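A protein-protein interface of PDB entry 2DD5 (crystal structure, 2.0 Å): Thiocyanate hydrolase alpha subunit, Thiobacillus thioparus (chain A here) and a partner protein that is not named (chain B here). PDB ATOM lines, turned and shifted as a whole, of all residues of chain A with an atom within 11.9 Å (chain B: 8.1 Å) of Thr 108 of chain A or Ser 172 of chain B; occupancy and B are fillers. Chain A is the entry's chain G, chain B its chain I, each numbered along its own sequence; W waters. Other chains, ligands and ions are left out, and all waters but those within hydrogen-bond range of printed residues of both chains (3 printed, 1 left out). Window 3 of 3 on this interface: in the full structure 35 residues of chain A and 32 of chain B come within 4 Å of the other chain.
The side-chain amide nitrogen (ND2) of Asn 111 of chain A is in hydrogen-bond range of the backbone carbonyl oxygen (O) of Glu 173 of chain B (2.9 Å). The side-chain carboxylate (OD1) of Asp 112 of chain A is in salt-bridge range of the guanidinium group (NH2) of Arg 160 of chain B, 2.9 Å away. The backbone NH (N) of Ile 176 of chain B sits at hydrogen-bond distance from the side-chain carboxylate (OD1) of Asp 112 of chain A (2.9 Å). NE2 of Gln 175 of chain B sits at hydrogen-bond distance from OG1 of Thr 113 of chain A (2.6 Å). N of Thr 113 of chain A sits at hydrogen-bond distance from O of Ile 176 of chain B, 2.9 Å away. OD1 of Asp 112 of chain A sits close to O of Val 174 of chain B, at 3.4 Å.
O of Asp 112 of chain A is in hydrogen-bond range of N of Gln 98 of chain A, 3.0 Å away. OD2 of Asp 112 of chain A lies within hydrogen-bond range of OH of Tyr 105 of chain A, at 2.6 Å. The side-chain hydroxyl (OG) of Ser 106 of chain A sits close to the backbone NH (N) of Thr 108 of chain A, at 3.1 Å. The backbone carbonyl oxygen (O) of Pro 171 of chain B sits at hydrogen-bond distance from the guanidinium group (NH1) of Arg 160 of chain B (3.1 Å). O of Ser 172 of chain B lies within hydrogen-bond range of NH2 of Arg 160 of chain B, 3.4 Å away. The guanidinium group (NH2) of Arg 160 of chain B lies within hydrogen-bond range of the backbone carbonyl oxygen (O) of Val 174 of chain B (2.7 Å).
Ser 172 of chain B touches Thr 108 of chain A (CB to O, 3.5 Å). CD1 of Phe 109 of chain A touches NE of Arg 160 of chain B, at 3.3 Å. Phe 109 of chain A touches Ser 172 of chain B (CE1 to CB, 3.7 Å). O of Asn 111 of chain A touches CG of Gln 175 of chain B, at 2.9 Å. C of Gln 175 of chain B touches OD1 of Asp 112 of chain A, 3.9 Å away.
Trp 102 of chain A touches none of the printed residues of chain B. Pro 103 of chain A touches none of the printed residues of chain B. Thr 108 of chain A touches just one residue of chain B: Ser 172. Of the printed residues of chain B, Asp 112 of chain A touches Arg 160, Val 174, Gln 175 and Ile 176. Ser 172 of chain B touches just these residues of chain A: Thr 108 (3.5 Å) and Phe 109 (3.7 Å). Of the printed residues of chain A, Glu 173 of chain B touches Asn 111 (2.9 Å). Val 174 of chain B touches just one residue of chain A: Asp 112. Printed residues of chain A within 4 Å of Gln 175 of chain B: Asn 111, Asp 112 and Thr 113.
Printed residues of chain B that touch a printed residue of chain A: Arg 160, Ser 172, Glu 173, Val 174, Gln 175 and Ile 176. Of the 14 printed residues of chain A, 5 touch a printed residue of chain B. Printed residues of chain A that touch a printed residue of chain B: Thr 108, Phe 109, Asn 111, Asp 112 and Thr 113. Among the printed residues, Asp or Glu carboxylates within 4 Å of a Lys or Arg side-chain nitrogen of the other chain: Asp 112 of chain A with Arg 160 of chain B (2.9 Å).
Water W1 lies within hydrogen-bond range of the backbone carbonyl oxygen (O) of Thr 108 of chain A and the side-chain hydroxyl (OG) of Ser 172 of chain B. Water W2 lies within hydrogen-bond range of O of Thr 113 of chain A, O of Ile 176 of chain B and NE2 of Gln 98 of chain A. Water W3 lies within hydrogen-bond range of N of Arg 160 of chain B and OH of Tyr 105 of chain A.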
ATOM      1  N   GLN A  98      30.597 -22.467 -19.456  1.00  0.00           N
ATOM      2  CA  GLN A  98      29.779 -22.293 -20.654  1.00  0.00           C
ATOM      3  C   GLN A  98      30.609 -22.274 -21.938  1.00  0.00           C
ATOM      4  O   GLN A  98      30.187 -22.809 -22.963  1.00  0.00           O
ATOM      5  CB  GLN A  98      28.947 -21.012 -20.543  1.00  0.00           C
ATOM      6  CG  GLN A  98      27.787 -21.125 -19.547  1.00  0.00           C
ATOM      7  CD  GLN A  98      26.631 -21.968 -20.068  1.00  0.00           C
ATOM      8  OE1 GLN A  98      26.829 -23.068 -20.587  1.00  0.00           O
ATOM      9  NE2 GLN A  98      25.414 -21.455 -19.922  1.00  0.00           N
ATOM     10  N   LYS A  99      31.793 -21.675 -21.880  1.00  0.00           N
ATOM     11  CA  LYS A  99      32.657 -21.608 -23.055  1.00  0.00           C
ATOM     12  C   LYS A  99      33.041 -22.998 -23.578  1.00  0.00           C
ATOM     13  O   LYS A  99      33.289 -23.165 -24.771  1.00  0.00           O
ATOM     14  CB  LYS A  99      33.927 -20.806 -22.741  1.00  0.00           C
ATOM     15  CG  LYS A  99      34.792 -21.420 -21.648  1.00  0.00           C
ATOM     16  CD  LYS A  99      36.127 -20.694 -21.496  1.00  0.00           C
ATOM     17  CE  LYS A  99      35.943 -19.243 -21.062  1.00  0.00           C
ATOM     18  NZ  LYS A  99      37.243 -18.511 -20.976  1.00  0.00           N
ATOM     19  N   TRP A 102      29.506 -24.239 -25.512  1.00  0.00           N
ATOM     20  CA  TRP A 102      29.098 -23.503 -26.703  1.00  0.00           C
ATOM     21  C   TRP A 102      30.229 -22.659 -27.284  1.00  0.00           C
ATOM     22  O   TRP A 102      30.681 -21.697 -26.667  1.00  0.00           O
ATOM     23  CB  TRP A 102      27.901 -22.613 -26.354  1.00  0.00           C
ATOM     24  CG  TRP A 102      27.015 -23.222 -25.296  1.00  0.00           C
ATOM     25  CD1 TRP A 102      26.917 -22.839 -23.986  1.00  0.00           C
ATOM     26  CD2 TRP A 102      26.133 -24.342 -25.453  1.00  0.00           C
ATOM     27  NE1 TRP A 102      26.028 -23.649 -23.318  1.00  0.00           N
ATOM     28  CE2 TRP A 102      25.532 -24.580 -24.194  1.00  0.00           C
ATOM     29  CE3 TRP A 102      25.792 -25.167 -26.534  1.00  0.00           C
ATOM     30  CZ2 TRP A 102      24.605 -25.610 -23.987  1.00  0.00           C
ATOM     31  CZ3 TRP A 102      24.870 -26.193 -26.329  1.00  0.00           C
ATOM     32  CH2 TRP A 102      24.286 -26.402 -25.060  1.00  0.00           C
ATOM     33  N   PRO A 103      30.686 -23.006 -28.497  1.00  0.00           N
ATOM     34  CA  PRO A 103      31.771 -22.301 -29.189  1.00  0.00           C
ATOM     35  C   PRO A 103      31.598 -20.790 -29.289  1.00  0.00           C
ATOM     36  O   PRO A 103      32.575 -20.042 -29.225  1.00  0.00           O
ATOM     37  CB  PRO A 103      31.781 -22.959 -30.569  1.00  0.00           C
ATOM     38  CG  PRO A 103      31.340 -24.356 -30.269  1.00  0.00           C
ATOM     39  CD  PRO A 103      30.192 -24.129 -29.314  1.00  0.00           C
ATOM     40  N   GLU A 104      30.357 -20.341 -29.434  1.00  0.00           N
ATOM     41  CA  GLU A 104      30.083 -18.918 -29.578  1.00  0.00           C
ATOM     42  C   GLU A 104      29.960 -18.111 -28.284  1.00  0.00           C
ATOM     43  O   GLU A 104      29.820 -16.891 -28.337  1.00  0.00           O
ATOM     44  CB  GLU A 104      28.814 -18.716 -30.417  1.00  0.00           C
ATOM     45  CG  GLU A 104      27.484 -18.851 -29.664  1.00  0.00           C
ATOM     46  CD  GLU A 104      27.088 -20.292 -29.330  1.00  0.00           C
ATOM     47  OE1 GLU A 104      27.787 -21.245 -29.744  1.00  0.00           O
ATOM     48  OE2 GLU A 104      26.054 -20.465 -28.648  1.00  0.00           O
ATOM     49  N   TYR A 105      30.010 -18.771 -27.129  1.00  0.00           N
ATOM     50  CA  TYR A 105      29.863 -18.051 -25.868  1.00  0.00           C
ATOM     51  C   TYR A 105      30.873 -16.903 -25.782  1.00  0.00           C
ATOM     52  O   TYR A 105      32.062 -17.086 -26.041  1.00  0.00           O
ATOM     53  CB  TYR A 105      30.027 -18.995 -24.673  1.00  0.00           C
ATOM     54  CG  TYR A 105      29.094 -18.651 -23.530  1.00  0.00           C
ATOM     55  CD1 TYR A 105      27.747 -19.012 -23.572  1.00  0.00           C
ATOM     56  CD2 TYR A 105      29.543 -17.918 -22.432  1.00  0.00           C
ATOM     57  CE1 TYR A 105      26.864 -18.646 -22.548  1.00  0.00           C
ATOM     58  CE2 TYR A 105      28.671 -17.547 -21.402  1.00  0.00           C
ATOM     59  CZ  TYR A 105      27.333 -17.915 -21.468  1.00  0.00           C
ATOM     60  OH  TYR A 105      26.464 -17.540 -20.463  1.00  0.00           O
ATOM     61  N   SER A 106      30.384 -15.723 -25.417  1.00  0.00           N
ATOM     62  CA  SER A 106      31.217 -14.526 -25.326  1.00  0.00           C
ATOM     63  C   SER A 106      32.195 -14.504 -24.153  1.00  0.00           C
ATOM     64  O   SER A 106      31.849 -14.888 -23.033  1.00  0.00           O
ATOM     65  CB  SER A 106      30.323 -13.289 -25.252  1.00  0.00           C
ATOM     66  OG  SER A 106      31.096 -12.122 -25.042  1.00  0.00           O
ATOM     67  N   ASP A 107      33.414 -14.039 -24.418  1.00  0.00           N
ATOM     68  CA  ASP A 107      34.436 -13.945 -23.381  1.00  0.00           C
ATOM     69  C   ASP A 107      34.029 -12.903 -22.353  1.00  0.00           C
ATOM     70  O   ASP A 107      34.532 -12.900 -21.231  1.00  0.00           O
ATOM     71  CB  ASP A 107      35.795 -13.556 -23.972  1.00  0.00           C
ATOM     72  CG  ASP A 107      36.356 -14.618 -24.889  1.00  0.00           C
ATOM     73  OD1 ASP A 107      36.187 -15.816 -24.575  1.00  0.00           O
ATOM     74  OD2 ASP A 107      36.980 -14.254 -25.912  1.00  0.00           O
ATOM     75  N   THR A 108      33.122 -12.013 -22.742  1.00  0.00           N
ATOM     76  CA  THR A 108      32.646 -10.979 -21.833  1.00  0.00           C
ATOM     77  C   THR A 108      32.012 -11.640 -20.610  1.00  0.00           C
ATOM     78  O   THR A 108      32.082 -11.112 -19.501  1.00  0.00           O
ATOM     79  CB  THR A 108      31.599 -10.079 -22.511  1.00  0.00           C
ATOM     80  OG1 THR A 108      32.229  -9.307 -23.539  1.00  0.00           O
ATOM     81  CG2 THR A 108      30.957  -9.137 -21.498  1.00  0.00           C
ATOM     82  N   PHE A 109      31.397 -12.799 -20.828  1.00  0.00           N
ATOM     83  CA  PHE A 109      30.748 -13.557 -19.761  1.00  0.00           C
ATOM     84  C   PHE A 109      31.570 -14.818 -19.498  1.00  0.00           C
ATOM     85  O   PHE A 109      31.052 -15.932 -19.513  1.00  0.00           O
ATOM     86  CB  PHE A 109      29.325 -13.933 -20.189  1.00  0.00           C
ATOM     87  CG  PHE A 109      28.506 -12.760 -20.651  1.00  0.00           C
ATOM     88  CD1 PHE A 109      28.281 -11.677 -19.804  1.00  0.00           C
ATOM     89  CD2 PHE A 109      27.973 -12.728 -21.939  1.00  0.00           C
ATOM     90  CE1 PHE A 109      27.541 -10.581 -20.225  1.00  0.00           C
ATOM     91  CE2 PHE A 109      27.228 -11.634 -22.373  1.00  0.00           C
ATOM     92  CZ  PHE A 109      27.011 -10.555 -21.515  1.00  0.00           C
ATOM     93  N   ALA A 110      32.859 -14.621 -19.239  1.00  0.00           N
ATOM     94  CA  ALA A 110      33.788 -15.723 -19.012  1.00  0.00           C
ATOM     95  C   ALA A 110      33.561 -16.586 -17.770  1.00  0.00           C
ATOM     96  O   ALA A 110      34.058 -17.704 -17.707  1.00  0.00           O
ATOM     97  CB  ALA A 110      35.217 -15.183 -19.002  1.00  0.00           C
ATOM     98  N   ASN A 111      32.816 -16.088 -16.792  1.00  0.00           N
ATOM     99  CA  ASN A 111      32.596 -16.861 -15.575  1.00  0.00           C
ATOM    100  C   ASN A 111      31.324 -17.702 -15.531  1.00  0.00           C
ATOM    101  O   ASN A 111      31.096 -18.428 -14.563  1.00  0.00           O
ATOM    102  CB  ASN A 111      32.633 -15.936 -14.358  1.00  0.00           C
ATOM    103  CG  ASN A 111      33.977 -15.249 -14.195  1.00  0.00           C
ATOM    104  OD1 ASN A 111      35.019 -15.865 -14.398  1.00  0.00           O
ATOM    105  ND2 ASN A 111      33.958 -13.976 -13.819  1.00  0.00           N
ATOM    106  N   ASP A 112      30.504 -17.626 -16.574  1.00  0.00           N
ATOM    107  CA  ASP A 112      29.254 -18.379 -16.592  1.00  0.00           C
ATOM    108  C   ASP A 112      29.456 -19.886 -16.637  1.00  0.00           C
ATOM    109  O   ASP A 112      30.356 -20.390 -17.305  1.00  0.00           O
ATOM    110  CB  ASP A 112      28.378 -17.929 -17.763  1.00  0.00           C
ATOM    111  CG  ASP A 112      27.853 -16.517 -17.584  1.00  0.00           C
ATOM    112  OD1 ASP A 112      28.105 -15.915 -16.517  1.00  0.00           O
ATOM    113  OD2 ASP A 112      27.181 -16.007 -18.506  1.00  0.00           O
ATOM    114  N   THR A 113      28.601 -20.604 -15.916  1.00  0.00           N
ATOM    115  CA  THR A 113      28.694 -22.053 -15.847  1.00  0.00           C
ATOM    116  C   THR A 113      27.343 -22.743 -15.999  1.00  0.00           C
ATOM    117  O   THR A 113      26.298 -22.099 -16.110  1.00  0.00           O
ATOM    118  CB  THR A 113      29.283 -22.498 -14.497  1.00  0.00           C
ATOM    119  OG1 THR A 113      28.478 -21.968 -13.438  1.00  0.00           O
ATOM    120  CG2 THR A 113      30.712 -22.002 -14.337  1.00  0.00           C
ATOM    121  N   ARG B 160      21.921 -15.454 -20.565  1.00  0.00           N
ATOM    122  CA  ARG B 160      21.937 -13.993 -20.457  1.00  0.00           C
ATOM    123  C   ARG B 160      20.813 -13.380 -21.279  1.00  0.00           C
ATOM    124  O   ARG B 160      20.135 -12.447 -20.839  1.00  0.00           O
ATOM    125  CB  ARG B 160      23.275 -13.438 -20.951  1.00  0.00           C
ATOM    126  CG  ARG B 160      24.488 -13.877 -20.137  1.00  0.00           C
ATOM    127  CD  ARG B 160      24.803 -12.884 -19.049  1.00  0.00           C
ATOM    128  NE  ARG B 160      25.901 -13.329 -18.196  1.00  0.00           N
ATOM    129  CZ  ARG B 160      26.367 -12.627 -17.169  1.00  0.00           C
ATOM    130  NH1 ARG B 160      25.830 -11.448 -16.880  1.00  0.00           N
ATOM    131  NH2 ARG B 160      27.349 -13.108 -16.419  1.00  0.00           N
ATOM    132  N   GLN B 169      19.074  -8.660 -15.590  1.00  0.00           N
ATOM    133  CA  GLN B 169      20.428  -8.524 -16.111  1.00  0.00           C
ATOM    134  C   GLN B 169      21.405  -8.473 -14.942  1.00  0.00           C
ATOM    135  O   GLN B 169      21.149  -7.790 -13.952  1.00  0.00           O
ATOM    136  CB  GLN B 169      20.539  -7.241 -16.937  1.00  0.00           C
ATOM    137  CG  GLN B 169      21.815  -7.113 -17.745  1.00  0.00           C
ATOM    138  CD  GLN B 169      21.824  -5.862 -18.611  1.00  0.00           C
ATOM    139  OE1 GLN B 169      22.050  -4.753 -18.120  1.00  0.00           O
ATOM    140  NE2 GLN B 169      21.565  -6.034 -19.904  1.00  0.00           N
ATOM    141  N   LEU B 170      22.508  -9.207 -15.052  1.00  0.00           N
ATOM    142  CA  LEU B 170      23.534  -9.226 -14.011  1.00  0.00           C
ATOM    143  C   LEU B 170      24.853  -8.723 -14.593  1.00  0.00           C
ATOM    144  O   LEU B 170      25.060  -8.772 -15.808  1.00  0.00           O
ATOM    145  CB  LEU B 170      23.752 -10.650 -13.478  1.00  0.00           C
ATOM    146  CG  LEU B 170      22.770 -11.293 -12.490  1.00  0.00           C
ATOM    147  CD1 LEU B 170      22.682 -10.437 -11.239  1.00  0.00           C
ATOM    148  CD2 LEU B 170      21.405 -11.446 -13.124  1.00  0.00           C
ATOM    149  N   PRO B 171      25.761  -8.219 -13.735  1.00  0.00           N
ATOM    150  CA  PRO B 171      27.051  -7.728 -14.227  1.00  0.00           C
ATOM    151  C   PRO B 171      27.722  -8.855 -15.005  1.00  0.00           C
ATOM    152  O   PRO B 171      27.517 -10.029 -14.696  1.00  0.00           O
ATOM    153  CB  PRO B 171      27.800  -7.376 -12.943  1.00  0.00           C
ATOM    154  CG  PRO B 171      26.689  -6.922 -12.036  1.00  0.00           C
ATOM    155  CD  PRO B 171      25.616  -7.966 -12.289  1.00  0.00           C
ATOM    156  N   SER B 172      28.517  -8.505 -16.009  1.00  0.00           N
ATOM    157  CA  SER B 172      29.178  -9.511 -16.828  1.00  0.00           C
ATOM    158  C   SER B 172      30.169 -10.376 -16.058  1.00  0.00           C
ATOM    159  O   SER B 172      30.410 -11.523 -16.431  1.00  0.00           O
ATOM    160  CB  SER B 172      29.885  -8.841 -18.011  1.00  0.00           C
ATOM    161  OG  SER B 172      30.907  -7.971 -17.563  1.00  0.00           O
ATOM    162  N   GLU B 173      30.739  -9.838 -14.984  1.00  0.00           N
ATOM    163  CA  GLU B 173      31.706 -10.597 -14.197  1.00  0.00           C
ATOM    164  C   GLU B 173      31.024 -11.585 -13.252  1.00  0.00           C
ATOM    165  O   GLU B 173      31.656 -12.515 -12.758  1.00  0.00           O
ATOM    166  CB  GLU B 173      32.603  -9.656 -13.381  1.00  0.00           C
ATOM    167  CG  GLU B 173      31.878  -8.902 -12.276  1.00  0.00           C
ATOM    168  CD  GLU B 173      31.316  -7.566 -12.733  1.00  0.00           C
ATOM    169  OE1 GLU B 173      31.111  -7.377 -13.957  1.00  0.00           O
ATOM    170  OE2 GLU B 173      31.070  -6.704 -11.857  1.00  0.00           O
ATOM    171  N   VAL B 174      29.738 -11.374 -12.992  1.00  0.00           N
ATOM    172  CA  VAL B 174      28.995 -12.269 -12.114  1.00  0.00           C
ATOM    173  C   VAL B 174      28.806 -13.607 -12.818  1.00  0.00           C
ATOM    174  O   VAL B 174      28.448 -13.656 -13.994  1.00  0.00           O
ATOM    175  CB  VAL B 174      27.605 -11.686 -11.761  1.00  0.00           C
ATOM    176  CG1 VAL B 174      26.745 -12.742 -11.086  1.00  0.00           C
ATOM    177  CG2 VAL B 174      27.767 -10.482 -10.842  1.00  0.00           C
ATOM    178  N   GLN B 175      29.065 -14.691 -12.100  1.00  0.00           N
ATOM    179  CA  GLN B 175      28.898 -16.023 -12.663  1.00  0.00           C
ATOM    180  C   GLN B 175      27.425 -16.417 -12.721  1.00  0.00           C
ATOM    181  O   GLN B 175      26.780 -16.585 -11.682  1.00  0.00           O
ATOM    182  CB  GLN B 175      29.646 -17.061 -11.819  1.00  0.00           C
ATOM    183  CG  GLN B 175      29.348 -18.504 -12.225  1.00  0.00           C
ATOM    184  CD  GLN B 175      29.930 -19.519 -11.259  1.00  0.00           C
ATOM    185  OE1 GLN B 175      30.651 -19.165 -10.323  1.00  0.00           O
ATOM    186  NE2 GLN B 175      29.621 -20.787 -11.482  1.00  0.00           N
ATOM    187  N   ILE B 176      26.876 -16.537 -13.925  1.00  0.00           N
ATOM    188  CA  ILE B 176      25.493 -16.984 -14.034  1.00  0.00           C
ATOM    189  C   ILE B 176      25.618 -18.494 -14.140  1.00  0.00           C
ATOM    190  O   ILE B 176      26.334 -18.998 -15.008  1.00  0.00           O
ATOM    191  CB  ILE B 176      24.781 -16.484 -15.313  1.00  0.00           C
ATOM    192  CG1 ILE B 176      24.557 -14.973 -15.250  1.00  0.00           C
ATOM    193  CG2 ILE B 176      23.437 -17.209 -15.463  1.00  0.00           C
ATOM    194  CD1 ILE B 176      23.568 -14.543 -14.198  1.00  0.00           C
HETATM  195  O   HOH W   1      33.498  -9.156 -18.292  1.00  0.00           O
HETATM  196  O   HOH W   2      25.402 -19.893 -17.405  1.00  0.00           O
HETATM  197  O   HOH W   3      24.308 -16.158 -22.065  1.00  0.00           O
